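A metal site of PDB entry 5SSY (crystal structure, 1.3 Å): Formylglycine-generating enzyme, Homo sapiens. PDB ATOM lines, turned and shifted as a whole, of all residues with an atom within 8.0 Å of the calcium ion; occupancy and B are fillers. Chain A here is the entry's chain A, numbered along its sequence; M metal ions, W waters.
NE of Arg 301 lies within salt-bridge range of OE1 of Glu 237 (2.8 Å). O of Glu 237 sits at hydrogen-bond distance from N of Lys 267 (2.9 Å). The side-chain carboxylate of Glu 237 lies within hydrogen-bond range of the indole nitrogen of Trp 168 (2.9 Å). The side-chain amide nitrogen of Asn 234 is in hydrogen-bond range of the side-chain carboxylate of Glu 67 (2.8 Å). The backbone carbonyl oxygen of Asn 230 sits close to the guanidinium group of Arg 301, at 3.4 Å. The backbone NH (N) of Gly 233 sits at hydrogen-bond distance from the backbone carbonyl oxygen (O) of Gly 268 (2.9 Å).
The calcium ion is bound by OE2 of Glu 237. O of Ala 235 is bound to the calcium ion, at 2.3 Å. The calcium ion is bound by OE2 of Glu 67, 2.4 Å away. O of Asn 230 is bound to the calcium ion (2.4 Å). The calcium ion is bound by water W1. The calcium ion is bound by O of Gly 233 (2.4 Å).
Residues that only touch the calcium ion: Ile 231. Of the 23 residues printed, 6 come within 4 Å of the calcium ion.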
ATOM      1  N   TYR A  66     -17.674  23.764  24.798  1.00  0.00           N
ATOM      2  CA  TYR A  66     -17.025  22.545  24.335  1.00  0.00           C
ATOM      3  C   TYR A  66     -15.737  22.891  23.612  1.00  0.00           C
ATOM      4  O   TYR A  66     -15.643  23.939  22.960  1.00  0.00           O
ATOM      5  CB  TYR A  66     -17.929  21.818  23.331  1.00  0.00           C
ATOM      6  CG  TYR A  66     -19.342  21.596  23.815  1.00  0.00           C
ATOM      7  CD1 TYR A  66     -19.611  20.688  24.825  1.00  0.00           C
ATOM      8  CD2 TYR A  66     -20.412  22.280  23.243  1.00  0.00           C
ATOM      9  CE1 TYR A  66     -20.898  20.459  25.272  1.00  0.00           C
ATOM     10  CE2 TYR A  66     -21.720  22.055  23.687  1.00  0.00           C
ATOM     11  CZ  TYR A  66     -21.945  21.140  24.702  1.00  0.00           C
ATOM     12  OH  TYR A  66     -23.226  20.921  25.157  1.00  0.00           O
ATOM     13  N   GLU A  67     -14.756  21.988  23.702  1.00  0.00           N
ATOM     14  CA  GLU A  67     -13.658  22.006  22.743  1.00  0.00           C
ATOM     15  C   GLU A  67     -14.240  21.998  21.337  1.00  0.00           C
ATOM     16  O   GLU A  67     -15.301  21.419  21.091  1.00  0.00           O
ATOM     17  CB  GLU A  67     -12.780  20.758  22.924  1.00  0.00           C
ATOM     18  CG  GLU A  67     -12.139  20.607  24.311  1.00  0.00           C
ATOM     19  CD  GLU A  67     -11.865  19.160  24.723  1.00  0.00           C
ATOM     20  OE1 GLU A  67     -12.661  18.251  24.404  1.00  0.00           O
ATOM     21  OE2 GLU A  67     -10.847  18.925  25.397  1.00  0.00           O
ATOM     22  N   PRO A 142     -12.999  16.117  19.915  1.00  0.00           N
ATOM     23  CA  PRO A 142     -12.262  17.365  19.663  1.00  0.00           C
ATOM     24  C   PRO A 142     -11.328  17.233  18.459  1.00  0.00           C
ATOM     25  O   PRO A 142     -10.698  16.189  18.242  1.00  0.00           O
ATOM     26  CB  PRO A 142     -11.468  17.580  20.962  1.00  0.00           C
ATOM     27  CG  PRO A 142     -11.338  16.182  21.544  1.00  0.00           C
ATOM     28  CD  PRO A 142     -12.655  15.547  21.228  1.00  0.00           C
ATOM     29  N   TRP A 168      -8.898  31.655  30.497  1.00  0.00           N
ATOM     30  CA  TRP A 168      -9.016  30.205  30.476  1.00  0.00           C
ATOM     31  C   TRP A 168      -8.985  29.633  31.886  1.00  0.00           C
ATOM     32  O   TRP A 168      -9.831  28.810  32.260  1.00  0.00           O
ATOM     33  CB  TRP A 168      -7.913  29.606  29.586  1.00  0.00           C
ATOM     34  CG  TRP A 168      -8.107  28.150  29.312  1.00  0.00           C
ATOM     35  CD1 TRP A 168      -8.614  27.596  28.172  1.00  0.00           C
ATOM     36  CD2 TRP A 168      -7.847  27.070  30.207  1.00  0.00           C
ATOM     37  NE1 TRP A 168      -8.664  26.218  28.299  1.00  0.00           N
ATOM     38  CE2 TRP A 168      -8.196  25.884  29.538  1.00  0.00           C
ATOM     39  CE3 TRP A 168      -7.321  26.989  31.505  1.00  0.00           C
ATOM     40  CZ2 TRP A 168      -8.060  24.635  30.123  1.00  0.00           C
ATOM     41  CZ3 TRP A 168      -7.216  25.741  32.083  1.00  0.00           C
ATOM     42  CH2 TRP A 168      -7.585  24.583  31.392  1.00  0.00           C
ATOM     43  N   ASN A 196     -11.384  13.078  31.231  1.00  0.00           N
ATOM     44  CA  ASN A 196     -10.762  12.026  30.421  1.00  0.00           C
ATOM     45  C   ASN A 196      -9.249  12.188  30.507  1.00  0.00           C
ATOM     46  O   ASN A 196      -8.676  13.044  29.824  1.00  0.00           O
ATOM     47  CB  ASN A 196     -11.227  12.129  28.980  1.00  0.00           C
ATOM     48  CG  ASN A 196     -10.585  11.086  28.083  1.00  0.00           C
ATOM     49  OD1 ASN A 196     -10.023  10.105  28.563  1.00  0.00           O
ATOM     50  ND2 ASN A 196     -10.677  11.281  26.788  1.00  0.00           N
ATOM     51  N   TYR A 229     -17.350  21.898  29.519  1.00  0.00           N
ATOM     52  CA  TYR A 229     -17.069  20.468  29.394  1.00  0.00           C
ATOM     53  C   TYR A 229     -15.610  20.245  29.017  1.00  0.00           C
ATOM     54  O   TYR A 229     -15.059  20.944  28.153  1.00  0.00           O
ATOM     55  CB  TYR A 229     -17.966  19.851  28.331  1.00  0.00           C
ATOM     56  CG  TYR A 229     -19.416  19.855  28.711  1.00  0.00           C
ATOM     57  CD1 TYR A 229     -20.193  20.994  28.568  1.00  0.00           C
ATOM     58  CD2 TYR A 229     -20.007  18.727  29.247  1.00  0.00           C
ATOM     59  CE1 TYR A 229     -21.540  20.989  28.916  1.00  0.00           C
ATOM     60  CE2 TYR A 229     -21.334  18.713  29.606  1.00  0.00           C
ATOM     61  CZ  TYR A 229     -22.084  19.845  29.452  1.00  0.00           C
ATOM     62  OH  TYR A 229     -23.409  19.786  29.807  1.00  0.00           O
ATOM     63  N   ASN A 230     -14.984  19.256  29.677  1.00  0.00           N
ATOM     64  CA  ASN A 230     -13.636  18.798  29.339  1.00  0.00           C
ATOM     65  C   ASN A 230     -12.616  19.907  29.353  1.00  0.00           C
ATOM     66  O   ASN A 230     -11.658  19.914  28.563  1.00  0.00           O
ATOM     67  CB  ASN A 230     -13.629  18.021  28.010  1.00  0.00           C
ATOM     68  CG  ASN A 230     -14.545  16.840  28.058  1.00  0.00           C
ATOM     69  OD1 ASN A 230     -14.311  15.884  28.797  1.00  0.00           O
ATOM     70  ND2 ASN A 230     -15.647  16.921  27.300  1.00  0.00           N
ATOM     71  N   ILE A 231     -12.797  20.867  30.251  1.00  0.00           N
ATOM     72  CA  ILE A 231     -11.838  21.960  30.375  1.00  0.00           C
ATOM     73  C   ILE A 231     -10.502  21.427  30.875  1.00  0.00           C
ATOM     74  O   ILE A 231      -9.443  21.905  30.456  1.00  0.00           O
ATOM     75  CB  ILE A 231     -12.424  23.117  31.226  1.00  0.00           C
ATOM     76  CG1 ILE A 231     -11.566  24.387  31.101  1.00  0.00           C
ATOM     77  CG2 ILE A 231     -12.615  22.703  32.678  1.00  0.00           C
ATOM     78  CD1 ILE A 231     -11.718  25.091  29.775  1.00  0.00           C
ATOM     79  N   VAL A 232     -10.515  20.420  31.744  1.00  0.00           N
ATOM     80  CA  VAL A 232      -9.312  19.634  32.010  1.00  0.00           C
ATOM     81  C   VAL A 232      -9.489  18.275  31.352  1.00  0.00           C
ATOM     82  O   VAL A 232     -10.596  17.737  31.282  1.00  0.00           O
ATOM     83  CB  VAL A 232      -8.840  19.509  33.475  1.00  0.00           C
ATOM     84  CG1 VAL A 232      -8.540  20.875  34.068  1.00  0.00           C
ATOM     85  CG2 VAL A 232      -9.854  18.722  34.310  1.00  0.00           C
ATOM     86  N   GLY A 233      -8.384  17.723  30.848  1.00  0.00           N
ATOM     87  CA  GLY A 233      -8.427  16.460  30.150  1.00  0.00           C
ATOM     88  C   GLY A 233      -8.959  16.549  28.722  1.00  0.00           C
ATOM     89  O   GLY A 233      -9.291  17.615  28.192  1.00  0.00           O
ATOM     90  N   ASN A 234      -9.061  15.366  28.099  1.00  0.00           N
ATOM     91  CA  ASN A 234      -9.475  15.211  26.719  1.00  0.00           C
ATOM     92  C   ASN A 234      -8.402  15.786  25.782  1.00  0.00           C
ATOM     93  O   ASN A 234      -7.361  15.159  25.604  1.00  0.00           O
ATOM     94  CB  ASN A 234     -10.872  15.775  26.469  1.00  0.00           C
ATOM     95  CG  ASN A 234     -11.677  14.914  25.522  1.00  0.00           C
ATOM     96  OD1 ASN A 234     -11.463  13.706  25.431  1.00  0.00           O
ATOM     97  ND2 ASN A 234     -12.610  15.529  24.813  1.00  0.00           N
ATOM     98  N   ALA A 235      -8.627  16.961  25.190  1.00  0.00           N
ATOM     99  CA  ALA A 235      -7.575  17.630  24.443  1.00  0.00           C
ATOM    100  C   ALA A 235      -7.009  18.770  25.289  1.00  0.00           C
ATOM    101  O   ALA A 235      -7.759  19.454  25.985  1.00  0.00           O
ATOM    102  CB  ALA A 235      -8.110  18.191  23.118  1.00  0.00           C
ATOM    103  N   TRP A 236      -5.691  18.956  25.211  1.00  0.00           N
ATOM    104  CA  TRP A 236      -5.067  20.211  25.609  1.00  0.00           C
ATOM    105  C   TRP A 236      -5.673  21.367  24.821  1.00  0.00           C
ATOM    106  O   TRP A 236      -6.243  21.198  23.737  1.00  0.00           O
ATOM    107  CB  TRP A 236      -3.578  20.189  25.226  1.00  0.00           C
ATOM    108  CG  TRP A 236      -2.626  19.524  26.199  1.00  0.00           C
ATOM    109  CD1 TRP A 236      -2.132  18.240  26.145  1.00  0.00           C
ATOM    110  CD2 TRP A 236      -2.000  20.132  27.341  1.00  0.00           C
ATOM    111  NE1 TRP A 236      -1.250  18.026  27.181  1.00  0.00           N
ATOM    112  CE2 TRP A 236      -1.167  19.162  27.939  1.00  0.00           C
ATOM    113  CE3 TRP A 236      -2.091  21.391  27.933  1.00  0.00           C
ATOM    114  CZ2 TRP A 236      -0.401  19.427  29.081  1.00  0.00           C
ATOM    115  CZ3 TRP A 236      -1.332  21.659  29.063  1.00  0.00           C
ATOM    116  CH2 TRP A 236      -0.517  20.671  29.633  1.00  0.00           C
ATOM    117  N   GLU A 237      -5.531  22.583  25.351  1.00  0.00           N
ATOM    118  CA  GLU A 237      -6.218  23.733  24.772  1.00  0.00           C
ATOM    119  C   GLU A 237      -5.289  24.921  24.634  1.00  0.00           C
ATOM    120  O   GLU A 237      -4.714  25.391  25.625  1.00  0.00           O
ATOM    121  CB  GLU A 237      -7.483  24.076  25.565  1.00  0.00           C
ATOM    122  CG  GLU A 237      -8.315  22.813  25.786  1.00  0.00           C
ATOM    123  CD  GLU A 237      -9.622  23.041  26.505  1.00  0.00           C
ATOM    124  OE1 GLU A 237     -10.014  24.211  26.738  1.00  0.00           O
ATOM    125  OE2 GLU A 237     -10.263  22.023  26.845  1.00  0.00           O
ATOM    126  N   LYS A 267      -3.201  24.859  27.984  1.00  0.00           N
ATOM    127  CA  LYS A 267      -3.715  24.559  29.316  1.00  0.00           C
ATOM    128  C   LYS A 267      -4.590  23.308  29.303  1.00  0.00           C
ATOM    129  O   LYS A 267      -5.149  22.912  28.279  1.00  0.00           O
ATOM    130  CB  LYS A 267      -4.575  25.711  29.857  1.00  0.00           C
ATOM    131  CG  LYS A 267      -3.864  27.069  29.941  1.00  0.00           C
ATOM    132  CD  LYS A 267      -3.029  27.190  31.223  1.00  0.00           C
ATOM    133  CE  LYS A 267      -3.879  27.537  32.443  1.00  0.00           C
ATOM    134  NZ  LYS A 267      -2.992  27.842  33.615  1.00  0.00           N
ATOM    135  N   GLY A 268      -4.701  22.703  30.476  1.00  0.00           N
ATOM    136  CA  GLY A 268      -5.782  21.784  30.782  1.00  0.00           C
ATOM    137  C   GLY A 268      -5.416  20.311  30.806  1.00  0.00           C
ATOM    138  O   GLY A 268      -6.171  19.518  31.379  1.00  0.00           O
ATOM    139  N   GLY A 269      -4.313  19.911  30.183  1.00  0.00           N
ATOM    140  CA  GLY A 269      -4.003  18.500  30.114  1.00  0.00           C
ATOM    141  C   GLY A 269      -4.931  17.765  29.148  1.00  0.00           C
ATOM    142  O   GLY A 269      -5.815  18.352  28.530  1.00  0.00           O
ATOM    143  N   SER A 270      -4.703  16.455  29.030  1.00  0.00           N
ATOM    144  CA  SER A 270      -5.317  15.672  27.969  1.00  0.00           C
ATOM    145  C   SER A 270      -5.577  14.240  28.440  1.00  0.00           C
ATOM    146  O   SER A 270      -5.264  13.855  29.575  1.00  0.00           O
ATOM    147  CB  SER A 270      -4.437  15.634  26.729  1.00  0.00           C
ATOM    148  OG  SER A 270      -3.311  14.807  26.939  1.00  0.00           O
ATOM    149  N   TYR A 271      -6.132  13.444  27.519  1.00  0.00           N
ATOM    150  CA  TYR A 271      -6.375  12.021  27.744  1.00  0.00           C
ATOM    151  C   TYR A 271      -5.098  11.240  28.018  1.00  0.00           C
ATOM    152  O   TYR A 271      -5.191  10.068  28.406  1.00  0.00           O
ATOM    153  CB  TYR A 271      -7.132  11.372  26.569  1.00  0.00           C
ATOM    154  CG  TYR A 271      -6.422  11.353  25.217  1.00  0.00           C
ATOM    155  CD1 TYR A 271      -5.579  10.306  24.851  1.00  0.00           C
ATOM    156  CD2 TYR A 271      -6.586  12.389  24.303  1.00  0.00           C
ATOM    157  CE1 TYR A 271      -4.925  10.302  23.606  1.00  0.00           C
ATOM    158  CE2 TYR A 271      -5.952  12.388  23.080  1.00  0.00           C
ATOM    159  CZ  TYR A 271      -5.129  11.344  22.735  1.00  0.00           C
ATOM    160  OH  TYR A 271      -4.498  11.356  21.508  1.00  0.00           O
ATOM    161  N   ASN A 297      -2.823  15.193  20.826  1.00  0.00           N
ATOM    162  CA  ASN A 297      -3.530  15.438  22.084  1.00  0.00           C
ATOM    163  C   ASN A 297      -3.822  16.911  22.320  1.00  0.00           C
ATOM    164  O   ASN A 297      -4.084  17.314  23.467  1.00  0.00           O
ATOM    165  CB  ASN A 297      -2.779  14.841  23.275  1.00  0.00           C
ATOM    166  CG  ASN A 297      -1.478  15.564  23.574  1.00  0.00           C
ATOM    167  OD1 ASN A 297      -0.957  16.296  22.737  1.00  0.00           O
ATOM    168  ND2 ASN A 297      -0.944  15.377  24.780  1.00  0.00           N
ATOM    169  N   GLY A 299      -5.881  20.450  21.117  1.00  0.00           N
ATOM    170  CA  GLY A 299      -6.981  21.116  20.465  1.00  0.00           C
ATOM    171  C   GLY A 299      -7.159  22.515  21.020  1.00  0.00           C
ATOM    172  O   GLY A 299      -6.184  23.173  21.408  1.00  0.00           O
ATOM    173  N   PHE A 300      -8.414  22.966  21.069  1.00  0.00           N
ATOM    174  CA  PHE A 300      -8.669  24.311  21.546  1.00  0.00           C
ATOM    175  C   PHE A 300     -10.170  24.532  21.693  1.00  0.00           C
ATOM    176  O   PHE A 300     -10.989  23.758  21.178  1.00  0.00           O
ATOM    177  CB  PHE A 300      -8.102  25.370  20.581  1.00  0.00           C
ATOM    178  CG  PHE A 300      -8.786  25.421  19.227  1.00  0.00           C
ATOM    179  CD1 PHE A 300      -8.560  24.427  18.293  1.00  0.00           C
ATOM    180  CD2 PHE A 300      -9.642  26.448  18.906  1.00  0.00           C
ATOM    181  CE1 PHE A 300      -9.183  24.458  17.049  1.00  0.00           C
ATOM    182  CE2 PHE A 300     -10.242  26.500  17.645  1.00  0.00           C
ATOM    183  CZ  PHE A 300     -10.017  25.482  16.730  1.00  0.00           C
ATOM    184  N   ARG A 301     -10.511  25.620  22.383  1.00  0.00           N
ATOM    185  CA  ARG A 301     -11.856  26.194  22.359  1.00  0.00           C
ATOM    186  C   ARG A 301     -11.744  27.709  22.214  1.00  0.00           C
ATOM    187  O   ARG A 301     -10.702  28.309  22.494  1.00  0.00           O
ATOM    188  CB  ARG A 301     -12.665  25.851  23.632  1.00  0.00           C
ATOM    189  CG  ARG A 301     -12.261  26.643  24.857  1.00  0.00           C
ATOM    190  CD  ARG A 301     -13.058  26.167  26.070  1.00  0.00           C
ATOM    191  NE  ARG A 301     -12.702  24.803  26.445  1.00  0.00           N
ATOM    192  CZ  ARG A 301     -13.555  23.875  26.846  1.00  0.00           C
ATOM    193  NH1 ARG A 301     -14.863  24.122  26.906  1.00  0.00           N
ATOM    194  NH2 ARG A 301     -13.097  22.674  27.168  1.00  0.00           N
HETATM  195 CA    CA M   1      -9.700  19.810  27.255  1.00  0.00          CA
HETATM  196  O   HOH W   1      -7.908  20.524  28.647  1.00  0.00           O
